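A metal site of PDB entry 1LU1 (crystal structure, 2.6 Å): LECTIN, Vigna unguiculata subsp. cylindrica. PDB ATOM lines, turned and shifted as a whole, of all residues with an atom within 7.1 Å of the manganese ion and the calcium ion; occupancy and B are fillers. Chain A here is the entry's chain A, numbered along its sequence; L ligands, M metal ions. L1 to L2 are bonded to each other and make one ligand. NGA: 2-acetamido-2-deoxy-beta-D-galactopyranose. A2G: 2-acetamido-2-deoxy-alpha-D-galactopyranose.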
ATOM      1  N   ASP A  85       4.441   9.548  25.347  1.00  0.00           N
ATOM      2  CA  ASP A  85       4.590  10.080  24.000  1.00  0.00           C
ATOM      3  C   ASP A  85       6.040  10.322  23.619  1.00  0.00           C
ATOM      4  O   ASP A  85       6.370  10.409  22.447  1.00  0.00           O
ATOM      5  CB  ASP A  85       3.817  11.399  23.871  1.00  0.00           C
ATOM      6  CG  ASP A  85       2.571  11.262  23.017  1.00  0.00           C
ATOM      7  OD1 ASP A  85       2.716  10.995  21.812  1.00  0.00           O
ATOM      8  OD2 ASP A  85       1.460  11.425  23.572  1.00  0.00           O
ATOM      9  N   GLY A  86       6.911  10.461  24.624  1.00  0.00           N
ATOM     10  CA  GLY A  86       8.317  10.683  24.342  1.00  0.00           C
ATOM     11  C   GLY A  86       8.949  11.755  25.202  1.00  0.00           C
ATOM     12  O   GLY A  86       8.270  12.453  25.945  1.00  0.00           O
ATOM     13  N   GLY A 102       0.785  16.021  24.928  1.00  0.00           N
ATOM     14  CA  GLY A 102       0.641  14.915  24.001  1.00  0.00           C
ATOM     15  C   GLY A 102       1.793  14.783  23.020  1.00  0.00           C
ATOM     16  O   GLY A 102       2.966  14.856  23.408  1.00  0.00           O
ATOM     17  N   GLY A 103       1.458  14.603  21.752  1.00  0.00           N
ATOM     18  CA  GLY A 103       2.467  14.439  20.715  1.00  0.00           C
ATOM     19  C   GLY A 103       3.345  15.638  20.447  1.00  0.00           C
ATOM     20  O   GLY A 103       4.235  15.570  19.591  1.00  0.00           O
ATOM     21  N   TYR A 104       3.107  16.737  21.144  1.00  0.00           N
ATOM     22  CA  TYR A 104       3.923  17.938  20.951  1.00  0.00           C
ATOM     23  C   TYR A 104       5.054  17.981  21.972  1.00  0.00           C
ATOM     24  O   TYR A 104       5.870  18.904  21.982  1.00  0.00           O
ATOM     25  CB  TYR A 104       3.044  19.194  21.042  1.00  0.00           C
ATOM     26  CG  TYR A 104       2.142  19.339  19.841  1.00  0.00           C
ATOM     27  CD1 TYR A 104       2.619  19.897  18.664  1.00  0.00           C
ATOM     28  CD2 TYR A 104       0.825  18.865  19.868  1.00  0.00           C
ATOM     29  CE1 TYR A 104       1.825  19.991  17.527  1.00  0.00           C
ATOM     30  CE2 TYR A 104       0.008  18.960  18.735  1.00  0.00           C
ATOM     31  CZ  TYR A 104       0.515  19.524  17.563  1.00  0.00           C
ATOM     32  OH  TYR A 104      -0.276  19.616  16.445  1.00  0.00           O
ATOM     33  N   LEU A 105       5.088  16.965  22.830  1.00  0.00           N
ATOM     34  CA  LEU A 105       6.129  16.819  23.848  1.00  0.00           C
ATOM     35  C   LEU A 105       6.352  18.040  24.730  1.00  0.00           C
ATOM     36  O   LEU A 105       7.390  18.171  25.369  1.00  0.00           O
ATOM     37  CB  LEU A 105       7.442  16.430  23.172  1.00  0.00           C
ATOM     38  CG  LEU A 105       7.379  15.229  22.217  1.00  0.00           C
ATOM     39  CD1 LEU A 105       8.721  15.045  21.508  1.00  0.00           C
ATOM     40  CD2 LEU A 105       7.014  13.973  23.018  1.00  0.00           C
ATOM     41  N   GLU A 123      14.416  14.851  19.823  1.00  0.00           N
ATOM     42  CA  GLU A 123      13.372  14.055  20.432  1.00  0.00           C
ATOM     43  C   GLU A 123      13.563  12.569  20.295  1.00  0.00           C
ATOM     44  O   GLU A 123      14.154  12.072  19.327  1.00  0.00           O
ATOM     45  CB  GLU A 123      12.026  14.398  19.823  1.00  0.00           C
ATOM     46  CG  GLU A 123      12.052  14.292  18.322  1.00  0.00           C
ATOM     47  CD  GLU A 123      10.698  14.035  17.724  1.00  0.00           C
ATOM     48  OE1 GLU A 123       9.917  14.998  17.553  1.00  0.00           O
ATOM     49  OE2 GLU A 123      10.404  12.858  17.429  1.00  0.00           O
ATOM     50  N   PHE A 124      13.021  11.872  21.283  1.00  0.00           N
ATOM     51  CA  PHE A 124      13.026  10.427  21.335  1.00  0.00           C
ATOM     52  C   PHE A 124      11.530  10.119  21.440  1.00  0.00           C
ATOM     53  O   PHE A 124      10.948   9.958  22.512  1.00  0.00           O
ATOM     54  CB  PHE A 124      13.842   9.973  22.548  1.00  0.00           C
ATOM     55  CG  PHE A 124      15.254  10.506  22.518  1.00  0.00           C
ATOM     56  CD1 PHE A 124      15.545  11.790  22.961  1.00  0.00           C
ATOM     57  CD2 PHE A 124      16.301   9.742  21.987  1.00  0.00           C
ATOM     58  CE1 PHE A 124      16.831  12.305  22.863  1.00  0.00           C
ATOM     59  CE2 PHE A 124      17.609  10.256  21.885  1.00  0.00           C
ATOM     60  CZ  PHE A 124      17.871  11.533  22.323  1.00  0.00           C
ATOM     61  N   ASP A 125      10.936  10.093  20.246  1.00  0.00           N
ATOM     62  CA  ASP A 125       9.523   9.872  19.994  1.00  0.00           C
ATOM     63  C   ASP A 125       9.081   8.413  20.108  1.00  0.00           C
ATOM     64  O   ASP A 125       9.452   7.607  19.263  1.00  0.00           O
ATOM     65  CB  ASP A 125       9.232  10.374  18.593  1.00  0.00           C
ATOM     66  CG  ASP A 125       7.825  10.849  18.424  1.00  0.00           C
ATOM     67  OD1 ASP A 125       6.942  10.330  19.146  1.00  0.00           O
ATOM     68  OD2 ASP A 125       7.605  11.719  17.556  1.00  0.00           O
ATOM     69  N   THR A 126       8.264   8.079  21.095  1.00  0.00           N
ATOM     70  CA  THR A 126       7.819   6.704  21.271  1.00  0.00           C
ATOM     71  C   THR A 126       6.424   6.401  20.708  1.00  0.00           C
ATOM     72  O   THR A 126       5.897   5.308  20.893  1.00  0.00           O
ATOM     73  CB  THR A 126       7.836   6.307  22.754  1.00  0.00           C
ATOM     74  OG1 THR A 126       6.865   7.074  23.464  1.00  0.00           O
ATOM     75  CG2 THR A 126       9.213   6.586  23.349  1.00  0.00           C
ATOM     76  N   LEU A 127       5.825   7.370  20.025  1.00  0.00           N
ATOM     77  CA  LEU A 127       4.498   7.178  19.429  1.00  0.00           C
ATOM     78  C   LEU A 127       4.398   7.939  18.111  1.00  0.00           C
ATOM     79  O   LEU A 127       4.593   9.160  18.052  1.00  0.00           O
ATOM     80  CB  LEU A 127       3.390   7.644  20.369  1.00  0.00           C
ATOM     81  CG  LEU A 127       1.981   7.465  19.793  1.00  0.00           C
ATOM     82  CD1 LEU A 127       1.338   6.222  20.387  1.00  0.00           C
ATOM     83  CD2 LEU A 127       1.146   8.684  20.076  1.00  0.00           C
ATOM     84  N   SER A 128       4.078   7.204  17.051  1.00  0.00           N
ATOM     85  CA  SER A 128       3.968   7.774  15.723  1.00  0.00           C
ATOM     86  C   SER A 128       2.655   8.529  15.506  1.00  0.00           C
ATOM     87  O   SER A 128       1.583   7.945  15.529  1.00  0.00           O
ATOM     88  CB  SER A 128       4.089   6.661  14.688  1.00  0.00           C
ATOM     89  OG  SER A 128       4.399   7.202  13.421  1.00  0.00           O
ATOM     90  N   ASN A 129       2.758   9.840  15.271  1.00  0.00           N
ATOM     91  CA  ASN A 129       1.579  10.655  15.023  1.00  0.00           C
ATOM     92  C   ASN A 129       1.416  10.801  13.510  1.00  0.00           C
ATOM     93  O   ASN A 129       2.167  11.526  12.862  1.00  0.00           O
ATOM     94  CB  ASN A 129       1.742  12.038  15.649  1.00  0.00           C
ATOM     95  CG  ASN A 129       2.006  11.971  17.139  1.00  0.00           C
ATOM     96  OD1 ASN A 129       3.152  12.096  17.580  1.00  0.00           O
ATOM     97  ND2 ASN A 129       0.955  11.786  17.917  1.00  0.00           N
ATOM     98  N   TRP A 132       2.749  13.811  11.047  1.00  0.00           N
ATOM     99  CA  TRP A 132       4.117  14.288  10.814  1.00  0.00           C
ATOM    100  C   TRP A 132       5.199  13.298  11.217  1.00  0.00           C
ATOM    101  O   TRP A 132       6.377  13.574  11.031  1.00  0.00           O
ATOM    102  CB  TRP A 132       4.352  15.571  11.609  1.00  0.00           C
ATOM    103  CG  TRP A 132       4.179  15.357  13.092  1.00  0.00           C
ATOM    104  CD1 TRP A 132       5.039  14.711  13.933  1.00  0.00           C
ATOM    105  CD2 TRP A 132       3.073  15.774  13.892  1.00  0.00           C
ATOM    106  NE1 TRP A 132       4.534  14.681  15.210  1.00  0.00           N
ATOM    107  CE2 TRP A 132       3.324  15.342  15.217  1.00  0.00           C
ATOM    108  CE3 TRP A 132       1.885  16.479  13.632  1.00  0.00           C
ATOM    109  CZ2 TRP A 132       2.440  15.570  16.266  1.00  0.00           C
ATOM    110  CZ3 TRP A 132       0.999  16.708  14.671  1.00  0.00           C
ATOM    111  CH2 TRP A 132       1.286  16.266  15.977  1.00  0.00           C
ATOM    112  N   ASP A 133       4.801  12.154  11.750  1.00  0.00           N
ATOM    113  CA  ASP A 133       5.774  11.171  12.218  1.00  0.00           C
ATOM    114  C   ASP A 133       6.068  10.026  11.266  1.00  0.00           C
ATOM    115  O   ASP A 133       5.217   9.620  10.471  1.00  0.00           O
ATOM    116  CB  ASP A 133       5.290  10.570  13.545  1.00  0.00           C
ATOM    117  CG  ASP A 133       5.839  11.298  14.751  1.00  0.00           C
ATOM    118  OD1 ASP A 133       6.703  12.180  14.551  1.00  0.00           O
ATOM    119  OD2 ASP A 133       5.405  10.992  15.888  1.00  0.00           O
ATOM    120  N   PRO A 134       7.290   9.486  11.343  1.00  0.00           N
ATOM    121  CA  PRO A 134       7.710   8.360  10.500  1.00  0.00           C
ATOM    122  C   PRO A 134       6.990   7.116  10.997  1.00  0.00           C
ATOM    123  O   PRO A 134       6.402   7.145  12.073  1.00  0.00           O
ATOM    124  CB  PRO A 134       9.221   8.266  10.744  1.00  0.00           C
ATOM    125  CG  PRO A 134       9.590   9.528  11.467  1.00  0.00           C
ATOM    126  CD  PRO A 134       8.381   9.937  12.215  1.00  0.00           C
ATOM    127  N   HIS A 138      11.262   6.612  16.885  1.00  0.00           N
ATOM    128  CA  HIS A 138      12.429   7.241  16.301  1.00  0.00           C
ATOM    129  C   HIS A 138      13.093   8.352  17.107  1.00  0.00           C
ATOM    130  O   HIS A 138      12.543   8.858  18.078  1.00  0.00           O
ATOM    131  CB  HIS A 138      12.007   7.845  14.981  1.00  0.00           C
ATOM    132  CG  HIS A 138      10.845   8.792  15.105  1.00  0.00           C
ATOM    133  ND1 HIS A 138       9.555   8.385  15.341  1.00  0.00           N
ATOM    134  CD2 HIS A 138      10.819  10.145  15.130  1.00  0.00           C
ATOM    135  CE1 HIS A 138       8.789   9.480  15.491  1.00  0.00           C
ATOM    136  NE2 HIS A 138       9.504  10.579  15.369  1.00  0.00           N
ATOM    137  N   ILE A 139      14.286   8.722  16.651  1.00  0.00           N
ATOM    138  CA  ILE A 139      15.064   9.787  17.242  1.00  0.00           C
ATOM    139  C   ILE A 139      15.000  10.831  16.136  1.00  0.00           C
ATOM    140  O   ILE A 139      15.121  10.485  14.968  1.00  0.00           O
ATOM    141  CB  ILE A 139      16.535   9.368  17.436  1.00  0.00           C
ATOM    142  CG1 ILE A 139      16.605   8.180  18.400  1.00  0.00           C
ATOM    143  CG2 ILE A 139      17.340  10.544  17.972  1.00  0.00           C
ATOM    144  CD1 ILE A 139      17.952   7.485  18.400  1.00  0.00           C
ATOM    145  N   GLY A 140      14.795  12.094  16.476  1.00  0.00           N
ATOM    146  CA  GLY A 140      14.704  13.084  15.431  1.00  0.00           C
ATOM    147  C   GLY A 140      15.203  14.442  15.859  1.00  0.00           C
ATOM    148  O   GLY A 140      15.262  14.739  17.046  1.00  0.00           O
ATOM    149  N   ASP A 142      14.381  18.291  15.777  1.00  0.00           N
ATOM    150  CA  ASP A 142      13.307  19.254  15.545  1.00  0.00           C
ATOM    151  C   ASP A 142      13.775  20.698  15.599  1.00  0.00           C
ATOM    152  O   ASP A 142      14.322  21.135  16.606  1.00  0.00           O
ATOM    153  CB  ASP A 142      12.196  19.071  16.572  1.00  0.00           C
ATOM    154  CG  ASP A 142      11.692  17.649  16.641  1.00  0.00           C
ATOM    155  OD1 ASP A 142      11.801  16.927  15.626  1.00  0.00           O
ATOM    156  OD2 ASP A 142      11.206  17.246  17.715  1.00  0.00           O
ATOM    157  N   ILE A 146       7.281  20.389  15.232  1.00  0.00           N
ATOM    158  CA  ILE A 146       7.289  19.026  15.756  1.00  0.00           C
ATOM    159  C   ILE A 146       7.597  18.000  14.650  1.00  0.00           C
ATOM    160  O   ILE A 146       7.767  16.807  14.924  1.00  0.00           O
ATOM    161  CB  ILE A 146       5.955  18.683  16.461  1.00  0.00           C
ATOM    162  CG1 ILE A 146       6.128  17.422  17.312  1.00  0.00           C
ATOM    163  CG2 ILE A 146       4.839  18.503  15.441  1.00  0.00           C
ATOM    164  CD1 ILE A 146       7.012  17.613  18.547  1.00  0.00           C
ATOM    165  N   LYS A 147       7.640  18.467  13.401  1.00  0.00           N
ATOM    166  CA  LYS A 147       7.959  17.585  12.280  1.00  0.00           C
ATOM    167  C   LYS A 147       9.482  17.645  12.159  1.00  0.00           C
ATOM    168  O   LYS A 147      10.037  18.651  11.709  1.00  0.00           O
ATOM    169  CB  LYS A 147       7.299  18.098  10.989  1.00  0.00           C
ATOM    170  CG  LYS A 147       7.128  17.030   9.929  1.00  0.00           C
ATOM    171  CD  LYS A 147       7.389  17.612   8.533  1.00  0.00           C
ATOM    172  CE  LYS A 147       6.312  17.188   7.527  1.00  0.00           C
ATOM    173  NZ  LYS A 147       4.930  17.523   8.036  1.00  0.00           N
ATOM    174  N   SER A 148      10.144  16.580  12.590  1.00  0.00           N
ATOM    175  CA  SER A 148      11.600  16.529  12.552  1.00  0.00           C
ATOM    176  C   SER A 148      12.168  16.742  11.150  1.00  0.00           C
ATOM    177  O   SER A 148      11.546  16.350  10.165  1.00  0.00           O
ATOM    178  CB  SER A 148      12.060  15.166  13.104  1.00  0.00           C
ATOM    179  OG  SER A 148      11.215  14.719  14.146  1.00  0.00           O
ATOM    180  N   THR A 151      15.244  11.982  10.829  1.00  0.00           N
ATOM    181  CA  THR A 151      14.948  10.977  11.852  1.00  0.00           C
ATOM    182  C   THR A 151      15.699   9.692  11.579  1.00  0.00           C
ATOM    183  O   THR A 151      16.276   9.541  10.512  1.00  0.00           O
ATOM    184  CB  THR A 151      13.465  10.614  11.907  1.00  0.00           C
ATOM    185  OG1 THR A 151      13.056  10.140  10.619  1.00  0.00           O
ATOM    186  CG2 THR A 151      12.629  11.822  12.292  1.00  0.00           C
HETATM  187  C1  NGA L   1      -6.636   9.420  17.668  1.00  0.00           C
HETATM  188  C2  NGA L   1      -5.221   9.745  18.128  1.00  0.00           C
HETATM  189  C3  NGA L   1      -5.263  10.788  19.209  1.00  0.00           C
HETATM  190  C4  NGA L   1      -6.137  11.992  18.881  1.00  0.00           C
HETATM  191  C5  NGA L   1      -7.488  11.535  18.372  1.00  0.00           C
HETATM  192  C6  NGA L   1      -8.395  12.687  17.911  1.00  0.00           C
HETATM  193  C7  NGA L   1      -3.415   8.184  18.102  1.00  0.00           C
HETATM  194  C8  NGA L   1      -2.810   6.920  18.665  1.00  0.00           C
HETATM  195  N2  NGA L   1      -4.571   8.547  18.628  1.00  0.00           N
HETATM  196  O1  NGA L   1      -6.544   8.626  16.534  1.00  0.00           O
HETATM  197  O3  NGA L   1      -3.919  11.259  19.454  1.00  0.00           O
HETATM  198  O4  NGA L   1      -5.453  12.778  17.914  1.00  0.00           O
HETATM  199  O5  NGA L   1      -7.291  10.621  17.273  1.00  0.00           O
HETATM  200  O7  NGA L   1      -2.827   8.865  17.225  1.00  0.00           O
HETATM  201  O5  A2G L   2      -3.637  10.581  21.783  1.00  0.00           O
HETATM  202  C1  A2G L   2      -3.595  11.644  20.801  1.00  0.00           C
HETATM  203  C2  A2G L   2      -2.235  12.371  20.857  1.00  0.00           C
HETATM  204  N2  A2G L   2      -2.153  13.329  19.771  1.00  0.00           N
HETATM  205  C3  A2G L   2      -1.058  11.393  20.767  1.00  0.00           C
HETATM  206  O3  A2G L   2       0.170  12.107  20.891  1.00  0.00           O
HETATM  207  C4  A2G L   2      -1.192  10.339  21.873  1.00  0.00           C
HETATM  208  O4  A2G L   2      -1.172  10.997  23.132  1.00  0.00           O
HETATM  209  C5  A2G L   2      -2.525   9.641  21.722  1.00  0.00           C
HETATM  210  C6  A2G L   2      -2.745   8.603  22.827  1.00  0.00           C
HETATM  211  O6  A2G L   2      -3.964   7.930  22.604  1.00  0.00           O
HETATM  212  C7  A2G L   2      -1.649  14.554  19.987  1.00  0.00           C
HETATM  213  O7  A2G L   2      -1.281  14.924  21.096  1.00  0.00           O
HETATM  214  C8  A2G L   2      -1.547  15.511  18.804  1.00  0.00           C
HETATM  215 MN    MN M   1       8.680  12.943  15.736  1.00  0.00          MN
HETATM  216 CA    CA M   2       5.053  11.471  18.244  1.00  0.00          CA
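Ser 148 touches the manganese ion.
The nearest printed residue that does not touch the manganese ion is Ile 146 (4.1 Å).
The calcium ion is bound by OD1 of Asn 129 (2.1 Å), O of Leu 127 (2.4 Å), OD1 of Asp 125 (2.4 Å), OD2 of Asp 133 (2.4 Å) and OD2 of Asp 125 (2.7 Å).
ND2 of Asn 129 sits at hydrogen-bond distance from O3 of A2G L2 (3.1 Å).
N of Gly 103 lies within hydrogen-bond range of O7 of A2G L2, 2.8 Å away.
OD2 of Asp 85 lies within hydrogen-bond range of O4 of A2G L2 (2.7 Å).
OG of Ser 148 lies within hydrogen-bond range of OD1 of Asp 142 (2.7 Å).
The side-chain carboxylate (OE1) of Glu 123 sits close to the side-chain carboxylate (OD2) of Asp 142 (2.6 Å).
OD1 of Asp 133 sits close to NE1 of Trp 132 (3.4 Å).
The backbone carbonyl oxygen of Gly 140 lies within hydrogen-bond range of the backbone NH of Glu 123.
The side-chain carboxylate (OE2) of Glu 123 is bound to the manganese ion (2.4 Å).
The side-chain carboxylate (OD1) of Asp 133 is bound to the manganese ion, 2.4 Å away.
The side-chain carboxylate (OD2) of Asp 125 binds the manganese ion.
The manganese ion is bound by NE2 of His 138 (2.5 Å).
The manganese ion has four donor atoms within binding distance.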
